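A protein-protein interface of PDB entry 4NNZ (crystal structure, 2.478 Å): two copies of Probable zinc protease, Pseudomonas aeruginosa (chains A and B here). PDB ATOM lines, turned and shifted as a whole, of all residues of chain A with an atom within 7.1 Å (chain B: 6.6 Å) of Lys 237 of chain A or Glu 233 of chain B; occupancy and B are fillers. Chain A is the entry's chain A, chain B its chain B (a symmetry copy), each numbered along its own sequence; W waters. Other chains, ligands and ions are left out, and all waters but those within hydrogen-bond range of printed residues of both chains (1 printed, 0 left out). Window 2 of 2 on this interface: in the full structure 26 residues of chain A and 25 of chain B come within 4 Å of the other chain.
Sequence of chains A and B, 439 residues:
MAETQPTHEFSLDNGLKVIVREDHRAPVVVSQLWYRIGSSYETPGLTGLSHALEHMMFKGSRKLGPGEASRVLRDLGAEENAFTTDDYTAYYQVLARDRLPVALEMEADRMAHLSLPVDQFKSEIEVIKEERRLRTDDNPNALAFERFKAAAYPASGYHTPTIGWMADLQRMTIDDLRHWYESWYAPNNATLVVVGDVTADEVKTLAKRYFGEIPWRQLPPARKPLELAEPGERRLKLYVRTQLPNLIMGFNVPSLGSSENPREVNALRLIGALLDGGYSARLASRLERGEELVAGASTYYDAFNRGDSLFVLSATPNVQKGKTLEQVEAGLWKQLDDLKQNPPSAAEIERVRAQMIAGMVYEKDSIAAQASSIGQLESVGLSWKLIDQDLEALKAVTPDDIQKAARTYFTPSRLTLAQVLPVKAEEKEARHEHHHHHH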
ATOM      1  N   ARG A 147       4.825  -1.301 -13.393  1.00  0.00           N
ATOM      2  CA  ARG A 147       5.923  -2.019 -13.959  1.00  0.00           C
ATOM      3  C   ARG A 147       7.253  -1.341 -13.783  1.00  0.00           C
ATOM      4  O   ARG A 147       8.228  -1.979 -13.557  1.00  0.00           O
ATOM      5  CB  ARG A 147       5.716  -2.200 -15.447  1.00  0.00           C
ATOM      6  CG  ARG A 147       4.388  -2.729 -15.903  1.00  0.00           C
ATOM      7  CD  ARG A 147       4.181  -4.127 -15.444  1.00  0.00           C
ATOM      8  NE  ARG A 147       2.827  -4.567 -15.608  1.00  0.00           N
ATOM      9  CZ  ARG A 147       2.384  -5.170 -16.684  1.00  0.00           C
ATOM     10  NH1 ARG A 147       3.171  -5.382 -17.695  1.00  0.00           N
ATOM     11  NH2 ARG A 147       1.154  -5.554 -16.738  1.00  0.00           N
ATOM     12  N   ARG A 235      16.145  -1.286 -19.076  1.00  0.00           N
ATOM     13  CA  ARG A 235      15.310  -0.590 -20.011  1.00  0.00           C
ATOM     14  C   ARG A 235      14.016  -1.350 -20.238  1.00  0.00           C
ATOM     15  O   ARG A 235      14.050  -2.507 -20.460  1.00  0.00           O
ATOM     16  CB  ARG A 235      16.074  -0.395 -21.303  1.00  0.00           C
ATOM     17  CG  ARG A 235      17.459   0.117 -21.056  1.00  0.00           C
ATOM     18  CD  ARG A 235      18.241   0.366 -22.308  1.00  0.00           C
ATOM     19  NE  ARG A 235      17.519   1.223 -23.194  1.00  0.00           N
ATOM     20  CZ  ARG A 235      17.686   2.522 -23.291  1.00  0.00           C
ATOM     21  NH1 ARG A 235      18.581   3.148 -22.561  1.00  0.00           N
ATOM     22  NH2 ARG A 235      16.930   3.174 -24.129  1.00  0.00           N
ATOM     23  N   LEU A 236      12.873  -0.675 -20.165  1.00  0.00           N
ATOM     24  CA  LEU A 236      11.559  -1.295 -20.353  1.00  0.00           C
ATOM     25  C   LEU A 236      10.838  -0.758 -21.546  1.00  0.00           C
ATOM     26  O   LEU A 236      10.941   0.375 -21.843  1.00  0.00           O
ATOM     27  CB  LEU A 236      10.655  -1.056 -19.178  1.00  0.00           C
ATOM     28  CG  LEU A 236      10.678  -2.071 -18.093  1.00  0.00           C
ATOM     29  CD1 LEU A 236      11.984  -1.893 -17.389  1.00  0.00           C
ATOM     30  CD2 LEU A 236       9.540  -1.794 -17.160  1.00  0.00           C
ATOM     31  N   LYS A 237      10.128  -1.614 -22.243  1.00  0.00           N
ATOM     32  CA  LYS A 237       9.265  -1.196 -23.304  1.00  0.00           C
ATOM     33  C   LYS A 237       7.890  -1.723 -23.057  1.00  0.00           C
ATOM     34  O   LYS A 237       7.715  -2.888 -22.956  1.00  0.00           O
ATOM     35  CB  LYS A 237       9.764  -1.743 -24.612  1.00  0.00           C
ATOM     36  CG  LYS A 237       9.397  -0.865 -25.774  1.00  0.00           C
ATOM     37  CD  LYS A 237       9.857  -1.440 -27.076  1.00  0.00           C
ATOM     38  CE  LYS A 237      11.240  -0.953 -27.379  1.00  0.00           C
ATOM     39  NZ  LYS A 237      11.463  -0.697 -28.824  1.00  0.00           N
ATOM     40  N   LEU A 238       6.915  -0.848 -22.941  1.00  0.00           N
ATOM     41  CA  LEU A 238       5.558  -1.244 -22.694  1.00  0.00           C
ATOM     42  C   LEU A 238       4.602  -0.652 -23.677  1.00  0.00           C
ATOM     43  O   LEU A 238       4.628   0.509 -23.919  1.00  0.00           O
ATOM     44  CB  LEU A 238       5.131  -0.789 -21.334  1.00  0.00           C
ATOM     45  CG  LEU A 238       5.853  -1.372 -20.163  1.00  0.00           C
ATOM     46  CD1 LEU A 238       5.880  -0.364 -19.042  1.00  0.00           C
ATOM     47  CD2 LEU A 238       5.113  -2.621 -19.764  1.00  0.00           C
ATOM     48  N   TYR A 239       3.724  -1.478 -24.192  1.00  0.00           N
ATOM     49  CA  TYR A 239       2.707  -1.024 -25.084  1.00  0.00           C
ATOM     50  C   TYR A 239       1.392  -0.972 -24.359  1.00  0.00           C
ATOM     51  O   TYR A 239       0.948  -1.930 -23.795  1.00  0.00           O
ATOM     52  CB  TYR A 239       2.614  -1.968 -26.249  1.00  0.00           C
ATOM     53  CG  TYR A 239       3.815  -1.933 -27.125  1.00  0.00           C
ATOM     54  CD1 TYR A 239       3.929  -0.999 -28.110  1.00  0.00           C
ATOM     55  CD2 TYR A 239       4.826  -2.827 -26.961  1.00  0.00           C
ATOM     56  CE1 TYR A 239       5.014  -0.960 -28.911  1.00  0.00           C
ATOM     57  CE2 TYR A 239       5.916  -2.793 -27.759  1.00  0.00           C
ATOM     58  CZ  TYR A 239       6.000  -1.853 -28.736  1.00  0.00           C
ATOM     59  OH  TYR A 239       7.088  -1.808 -29.528  1.00  0.00           O
ATOM     60  N   GLU A 326      13.855   8.118 -28.357  1.00  0.00           N
ATOM     61  CA  GLU A 326      15.287   8.016 -28.325  1.00  0.00           C
ATOM     62  C   GLU A 326      15.974   9.359 -28.294  1.00  0.00           C
ATOM     63  O   GLU A 326      16.957   9.521 -27.642  1.00  0.00           O
ATOM     64  CB  GLU A 326      15.768   7.176 -29.473  1.00  0.00           C
ATOM     65  CG  GLU A 326      15.447   5.712 -29.311  1.00  0.00           C
ATOM     66  CD  GLU A 326      14.008   5.392 -29.596  1.00  0.00           C
ATOM     67  OE1 GLU A 326      13.404   6.050 -30.431  1.00  0.00           O
ATOM     68  OE2 GLU A 326      13.485   4.466 -28.992  1.00  0.00           O
ATOM     69  N   LEU A 417      14.877   2.910 -17.147  1.00  0.00           N
ATOM     70  CA  LEU A 417      14.237   3.712 -18.145  1.00  0.00           C
ATOM     71  C   LEU A 417      13.133   2.929 -18.808  1.00  0.00           C
ATOM     72  O   LEU A 417      13.328   1.823 -19.183  1.00  0.00           O
ATOM     73  CB  LEU A 417      15.251   4.148 -19.182  1.00  0.00           C
ATOM     74  CG  LEU A 417      14.716   4.811 -20.424  1.00  0.00           C
ATOM     75  CD1 LEU A 417      15.723   5.743 -21.003  1.00  0.00           C
ATOM     76  CD2 LEU A 417      14.291   3.799 -21.440  1.00  0.00           C
ATOM     77  N   ALA A 418      11.962   3.518 -18.944  1.00  0.00           N
ATOM     78  CA  ALA A 418      10.869   2.850 -19.604  1.00  0.00           C
ATOM     79  C   ALA A 418      10.219   3.633 -20.720  1.00  0.00           C
ATOM     80  O   ALA A 418       9.921   4.754 -20.544  1.00  0.00           O
ATOM     81  CB  ALA A 418       9.835   2.457 -18.597  1.00  0.00           C
ATOM     82  N   GLN A 419       9.965   3.002 -21.851  1.00  0.00           N
ATOM     83  CA  GLN A 419       9.250   3.625 -22.935  1.00  0.00           C
ATOM     84  C   GLN A 419       7.831   3.154 -22.892  1.00  0.00           C
ATOM     85  O   GLN A 419       7.578   1.988 -22.891  1.00  0.00           O
ATOM     86  CB  GLN A 419       9.875   3.268 -24.275  1.00  0.00           C
ATOM     87  CG  GLN A 419      11.369   3.483 -24.310  1.00  0.00           C
ATOM     88  CD  GLN A 419      11.990   3.542 -25.683  1.00  0.00           C
ATOM     89  OE1 GLN A 419      11.593   2.873 -26.600  1.00  0.00           O
ATOM     90  NE2 GLN A 419      13.009   4.331 -25.801  1.00  0.00           N
ATOM     91  N   VAL A 420       6.905   4.079 -22.823  1.00  0.00           N
ATOM     92  CA  VAL A 420       5.535   3.700 -22.825  1.00  0.00           C
ATOM     93  C   VAL A 420       4.964   4.045 -24.154  1.00  0.00           C
ATOM     94  O   VAL A 420       4.905   5.172 -24.513  1.00  0.00           O
ATOM     95  CB  VAL A 420       4.766   4.440 -21.757  1.00  0.00           C
ATOM     96  CG1 VAL A 420       3.388   3.873 -21.624  1.00  0.00           C
ATOM     97  CG2 VAL A 420       5.493   4.379 -20.448  1.00  0.00           C
ATOM     98  N   LEU A 421       4.570   3.044 -24.892  1.00  0.00           N
ATOM     99  CA  LEU A 421       4.185   3.264 -26.242  1.00  0.00           C
ATOM    100  C   LEU A 421       2.776   2.930 -26.540  1.00  0.00           C
ATOM    101  O   LEU A 421       2.203   2.063 -25.964  1.00  0.00           O
ATOM    102  CB  LEU A 421       5.085   2.499 -27.177  1.00  0.00           C
ATOM    103  CG  LEU A 421       6.507   2.985 -27.192  1.00  0.00           C
ATOM    104  CD1 LEU A 421       7.337   1.991 -27.940  1.00  0.00           C
ATOM    105  CD2 LEU A 421       6.593   4.315 -27.860  1.00  0.00           C
ATOM    106  N   GLU B 230       2.245 -11.261 -18.824  1.00  0.00           N
ATOM    107  CA  GLU B 230       2.998 -10.464 -19.754  1.00  0.00           C
ATOM    108  C   GLU B 230       3.587  -9.227 -19.121  1.00  0.00           C
ATOM    109  O   GLU B 230       3.081  -8.142 -19.273  1.00  0.00           O
ATOM    110  CB  GLU B 230       2.141 -10.092 -20.939  1.00  0.00           C
ATOM    111  CG  GLU B 230       1.915 -11.220 -21.909  1.00  0.00           C
ATOM    112  CD  GLU B 230       0.836 -10.935 -22.917  1.00  0.00           C
ATOM    113  OE1 GLU B 230      -0.324 -10.859 -22.533  1.00  0.00           O
ATOM    114  OE2 GLU B 230       1.129 -10.815 -24.105  1.00  0.00           O
ATOM    115  N   PRO B 231       4.689  -9.371 -18.417  1.00  0.00           N
ATOM    116  CA  PRO B 231       5.301  -8.262 -17.693  1.00  0.00           C
ATOM    117  C   PRO B 231       5.743  -7.120 -18.578  1.00  0.00           C
ATOM    118  O   PRO B 231       5.728  -5.994 -18.177  1.00  0.00           O
ATOM    119  CB  PRO B 231       6.503  -8.901 -17.051  1.00  0.00           C
ATOM    120  CG  PRO B 231       6.139 -10.301 -16.905  1.00  0.00           C
ATOM    121  CD  PRO B 231       5.325 -10.641 -18.086  1.00  0.00           C
ATOM    122  N   GLY B 232       6.112  -7.430 -19.799  1.00  0.00           N
ATOM    123  CA  GLY B 232       6.666  -6.472 -20.705  1.00  0.00           C
ATOM    124  C   GLY B 232       8.106  -6.753 -20.995  1.00  0.00           C
ATOM    125  O   GLY B 232       8.739  -7.444 -20.283  1.00  0.00           O
ATOM    126  N   GLU B 233       8.609  -6.190 -22.070  1.00  0.00           N
ATOM    127  CA  GLU B 233       9.933  -6.444 -22.538  1.00  0.00           C
ATOM    128  C   GLU B 233      10.857  -5.718 -21.631  1.00  0.00           C
ATOM    129  O   GLU B 233      10.769  -4.547 -21.519  1.00  0.00           O
ATOM    130  CB  GLU B 233      10.040  -5.847 -23.922  1.00  0.00           C
ATOM    131  CG  GLU B 233      11.233  -6.207 -24.769  1.00  0.00           C
ATOM    132  CD  GLU B 233      11.195  -5.550 -26.137  1.00  0.00           C
ATOM    133  OE1 GLU B 233      10.208  -5.688 -26.854  1.00  0.00           O
ATOM    134  OE2 GLU B 233      12.150  -4.873 -26.511  1.00  0.00           O
ATOM    135  N   ARG B 234      11.755  -6.416 -20.978  1.00  0.00           N
ATOM    136  CA  ARG B 234      12.770  -5.755 -20.208  1.00  0.00           C
ATOM    137  C   ARG B 234      14.173  -6.164 -20.622  1.00  0.00           C
ATOM    138  O   ARG B 234      14.439  -7.288 -20.906  1.00  0.00           O
ATOM    139  CB  ARG B 234      12.528  -5.904 -18.710  1.00  0.00           C
ATOM    140  CG  ARG B 234      12.066  -7.245 -18.258  1.00  0.00           C
ATOM    141  CD  ARG B 234      10.720  -7.204 -17.602  1.00  0.00           C
ATOM    142  NE  ARG B 234       9.888  -8.150 -18.298  1.00  0.00           N
ATOM    143  CZ  ARG B 234       9.740  -9.405 -17.959  1.00  0.00           C
ATOM    144  NH1 ARG B 234      10.310  -9.845 -16.896  1.00  0.00           N
ATOM    145  NH2 ARG B 234       9.015 -10.198 -18.679  1.00  0.00           N
ATOM    146  N   ARG B 235      15.055  -5.202 -20.692  1.00  0.00           N
ATOM    147  CA  ARG B 235      16.369  -5.428 -21.190  1.00  0.00           C
ATOM    148  C   ARG B 235      17.368  -4.895 -20.226  1.00  0.00           C
ATOM    149  O   ARG B 235      17.203  -3.855 -19.709  1.00  0.00           O
ATOM    150  CB  ARG B 235      16.505  -4.739 -22.517  1.00  0.00           C
ATOM    151  CG  ARG B 235      15.665  -5.369 -23.578  1.00  0.00           C
ATOM    152  CD  ARG B 235      15.660  -4.535 -24.818  1.00  0.00           C
ATOM    153  NE  ARG B 235      16.959  -4.570 -25.427  1.00  0.00           N
ATOM    154  CZ  ARG B 235      17.359  -5.511 -26.245  1.00  0.00           C
ATOM    155  NH1 ARG B 235      16.556  -6.490 -26.566  1.00  0.00           N
ATOM    156  NH2 ARG B 235      18.564  -5.461 -26.724  1.00  0.00           N
ATOM    157  N   GLU B 329      21.474 -12.184 -30.568  1.00  0.00           N
ATOM    158  CA  GLU B 329      20.074 -12.089 -30.277  1.00  0.00           C
ATOM    159  C   GLU B 329      19.229 -12.369 -31.475  1.00  0.00           C
ATOM    160  O   GLU B 329      18.276 -13.081 -31.400  1.00  0.00           O
ATOM    161  CB  GLU B 329      19.771 -10.697 -29.788  1.00  0.00           C
ATOM    162  CG  GLU B 329      18.394 -10.502 -29.213  1.00  0.00           C
ATOM    163  CD  GLU B 329      18.121  -9.064 -28.895  1.00  0.00           C
ATOM    164  OE1 GLU B 329      19.081  -8.322 -28.695  1.00  0.00           O
ATOM    165  OE2 GLU B 329      16.957  -8.685 -28.836  1.00  0.00           O
ATOM    166  N   PRO B 412       7.971 -10.880 -27.047  1.00  0.00           N
ATOM    167  CA  PRO B 412       8.751  -9.832 -26.418  1.00  0.00           C
ATOM    168  C   PRO B 412       8.127  -9.347 -25.139  1.00  0.00           C
ATOM    169  O   PRO B 412       8.820  -8.913 -24.281  1.00  0.00           O
ATOM    170  CB  PRO B 412       8.754  -8.758 -27.465  1.00  0.00           C
ATOM    171  CG  PRO B 412       8.697  -9.481 -28.718  1.00  0.00           C
ATOM    172  CD  PRO B 412       7.988 -10.757 -28.500  1.00  0.00           C
ATOM    173  N   SER B 413       6.826  -9.438 -25.030  1.00  0.00           N
ATOM    174  CA  SER B 413       6.134  -9.042 -23.838  1.00  0.00           C
ATOM    175  C   SER B 413       6.352  -9.999 -22.689  1.00  0.00           C
ATOM    176  O   SER B 413       5.983  -9.724 -21.600  1.00  0.00           O
ATOM    177  CB  SER B 413       4.655  -8.840 -24.109  1.00  0.00           C
ATOM    178  OG  SER B 413       3.982 -10.038 -24.353  1.00  0.00           O
ATOM    179  N   ARG B 414       6.925 -11.149 -22.961  1.00  0.00           N
ATOM    180  CA  ARG B 414       7.304 -12.060 -21.920  1.00  0.00           C
ATOM    181  C   ARG B 414       8.796 -12.146 -21.640  1.00  0.00           C
ATOM    182  O   ARG B 414       9.218 -12.955 -20.894  1.00  0.00           O
ATOM    183  CB  ARG B 414       6.718 -13.419 -22.213  1.00  0.00           C
ATOM    184  CG  ARG B 414       5.227 -13.431 -22.116  1.00  0.00           C
ATOM    185  CD  ARG B 414       4.676 -14.604 -22.867  1.00  0.00           C
ATOM    186  NE  ARG B 414       3.305 -14.846 -22.533  1.00  0.00           N
ATOM    187  CZ  ARG B 414       2.299 -14.508 -23.298  1.00  0.00           C
ATOM    188  NH1 ARG B 414       2.526 -13.945 -24.449  1.00  0.00           N
ATOM    189  NH2 ARG B 414       1.072 -14.756 -22.913  1.00  0.00           N
ATOM    190  N   LEU B 415       9.575 -11.290 -22.255  1.00  0.00           N
ATOM    191  CA  LEU B 415      10.981 -11.500 -22.378  1.00  0.00           C
ATOM    192  C   LEU B 415      11.727 -10.567 -21.465  1.00  0.00           C
ATOM    193  O   LEU B 415      11.406  -9.429 -21.329  1.00  0.00           O
ATOM    194  CB  LEU B 415      11.437 -11.304 -23.800  1.00  0.00           C
ATOM    195  CG  LEU B 415      12.898 -10.959 -24.036  1.00  0.00           C
ATOM    196  CD1 LEU B 415      13.755 -12.192 -24.114  1.00  0.00           C
ATOM    197  CD2 LEU B 415      12.955 -10.239 -25.337  1.00  0.00           C
ATOM    198  N   THR B 416      12.732 -11.100 -20.815  1.00  0.00           N
ATOM    199  CA  THR B 416      13.695 -10.280 -20.156  1.00  0.00           C
ATOM    200  C   THR B 416      15.056 -10.661 -20.679  1.00  0.00           C
ATOM    201  O   THR B 416      15.354 -11.795 -20.792  1.00  0.00           O
ATOM    202  CB  THR B 416      13.503 -10.277 -18.604  1.00  0.00           C
ATOM    203  OG1 THR B 416      14.746 -10.277 -17.921  1.00  0.00           O
ATOM    204  CG2 THR B 416      12.674 -11.414 -18.113  1.00  0.00           C
ATOM    205  N   LEU B 417      15.819  -9.687 -21.115  1.00  0.00           N
ATOM    206  CA  LEU B 417      17.026  -9.950 -21.831  1.00  0.00           C
ATOM    207  C   LEU B 417      18.135  -9.232 -21.159  1.00  0.00           C
ATOM    208  O   LEU B 417      18.012  -8.095 -20.841  1.00  0.00           O
ATOM    209  CB  LEU B 417      16.914  -9.498 -23.267  1.00  0.00           C
ATOM    210  CG  LEU B 417      18.116  -9.705 -24.181  1.00  0.00           C
ATOM    211  CD1 LEU B 417      17.711 -10.041 -25.585  1.00  0.00           C
ATOM    212  CD2 LEU B 417      19.025  -8.516 -24.176  1.00  0.00           C
HETATM  213  O   HOH W   1       6.388  -5.022 -24.156  1.00  0.00           O
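The backbone carbonyl oxygen of Glu 230 of chain B lies within hydrogen-bond range of the guanidinium group of Arg 147 of chain A. O of Pro 231 of chain B sits at hydrogen-bond distance from NH1 of Arg 147 of chain A (2.7 Å). The backbone NH of Arg 235 of chain A sits at hydrogen-bond distance from the backbone carbonyl oxygen of Arg 235 of chain B, at 2.8 Å. The backbone NH (N) of Lys 237 of chain A lies within hydrogen-bond range of the backbone carbonyl oxygen (O) of Glu 233 of chain B (3.1 Å).
The backbone NH (N) of Leu 236 of chain A is in hydrogen-bond range of the backbone carbonyl oxygen (O) of Leu 417 of chain A (2.7 Å). N of Leu 238 of chain A sits at hydrogen-bond distance from O of Gln 419 of chain A, 2.9 Å away. The backbone carbonyl oxygen of Leu 238 of chain A sits at hydrogen-bond distance from the backbone NH of Leu 421 of chain A. OE2 of Glu 230 of chain B is in hydrogen-bond range of OG of Ser 413 of chain B (3.0 Å). OE2 of Glu 230 of chain B is in salt-bridge range of NH1 of Arg 414 of chain B (3.4 Å). NH1 of Arg 235 of chain B lies within salt-bridge range of OE2 of Glu 329 of chain B, at 3.2 Å.
Among the printed residues, pairs that only touch across the chains: Arg 235 of chain A with Arg 234 of chain B, Leu 236 of chain A with Glu 233 of chain B and Leu 238 of chain A with Pro 231 of chain B.
Lys 237 of chain A touches just one residue of chain B: Glu 233 (3.1 Å). Printed residues of chain A within 4 Å of Glu 233 of chain B: Leu 236 (3.5 Å) and Lys 237 (3.1 Å). Printed residues of chain B within 4 Å of Arg 147 of chain A: Glu 230 and Pro 231. Of the printed residues of chain A, Glu 230 of chain B touches Arg 147 (3.2 Å). The nearest printed residue of chain A that does not touch Glu 233 of chain B is Arg 235 of chain A (4.01 Å).
Of the 12 printed residues of chain A, 5 touch a printed residue of chain B. Hydrophobic or aromatic side chains of chain A within 4 Å of the printed part of chain B: Leu 238. Along chain A the printed residues that touch a printed residue of chain B span positions 147 to 238. Of the 13 printed residues of chain B, 5 touch a printed residue of chain A. Along chain B the printed residues that touch a printed residue of chain A span positions 230 to 235.
Arg 235 of chain A touches its own counterpart, Arg 235 of chain B. 2 positions are printed for both chains. Of the 7 pairs that touch across the chains among the printed residues, 1 has its exchanged pair printed and touching as well.
Water W1 bridges O of Lys 237 of chain A (2.8 Å) and N of Glu 233 of chain B (3.3 Å).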
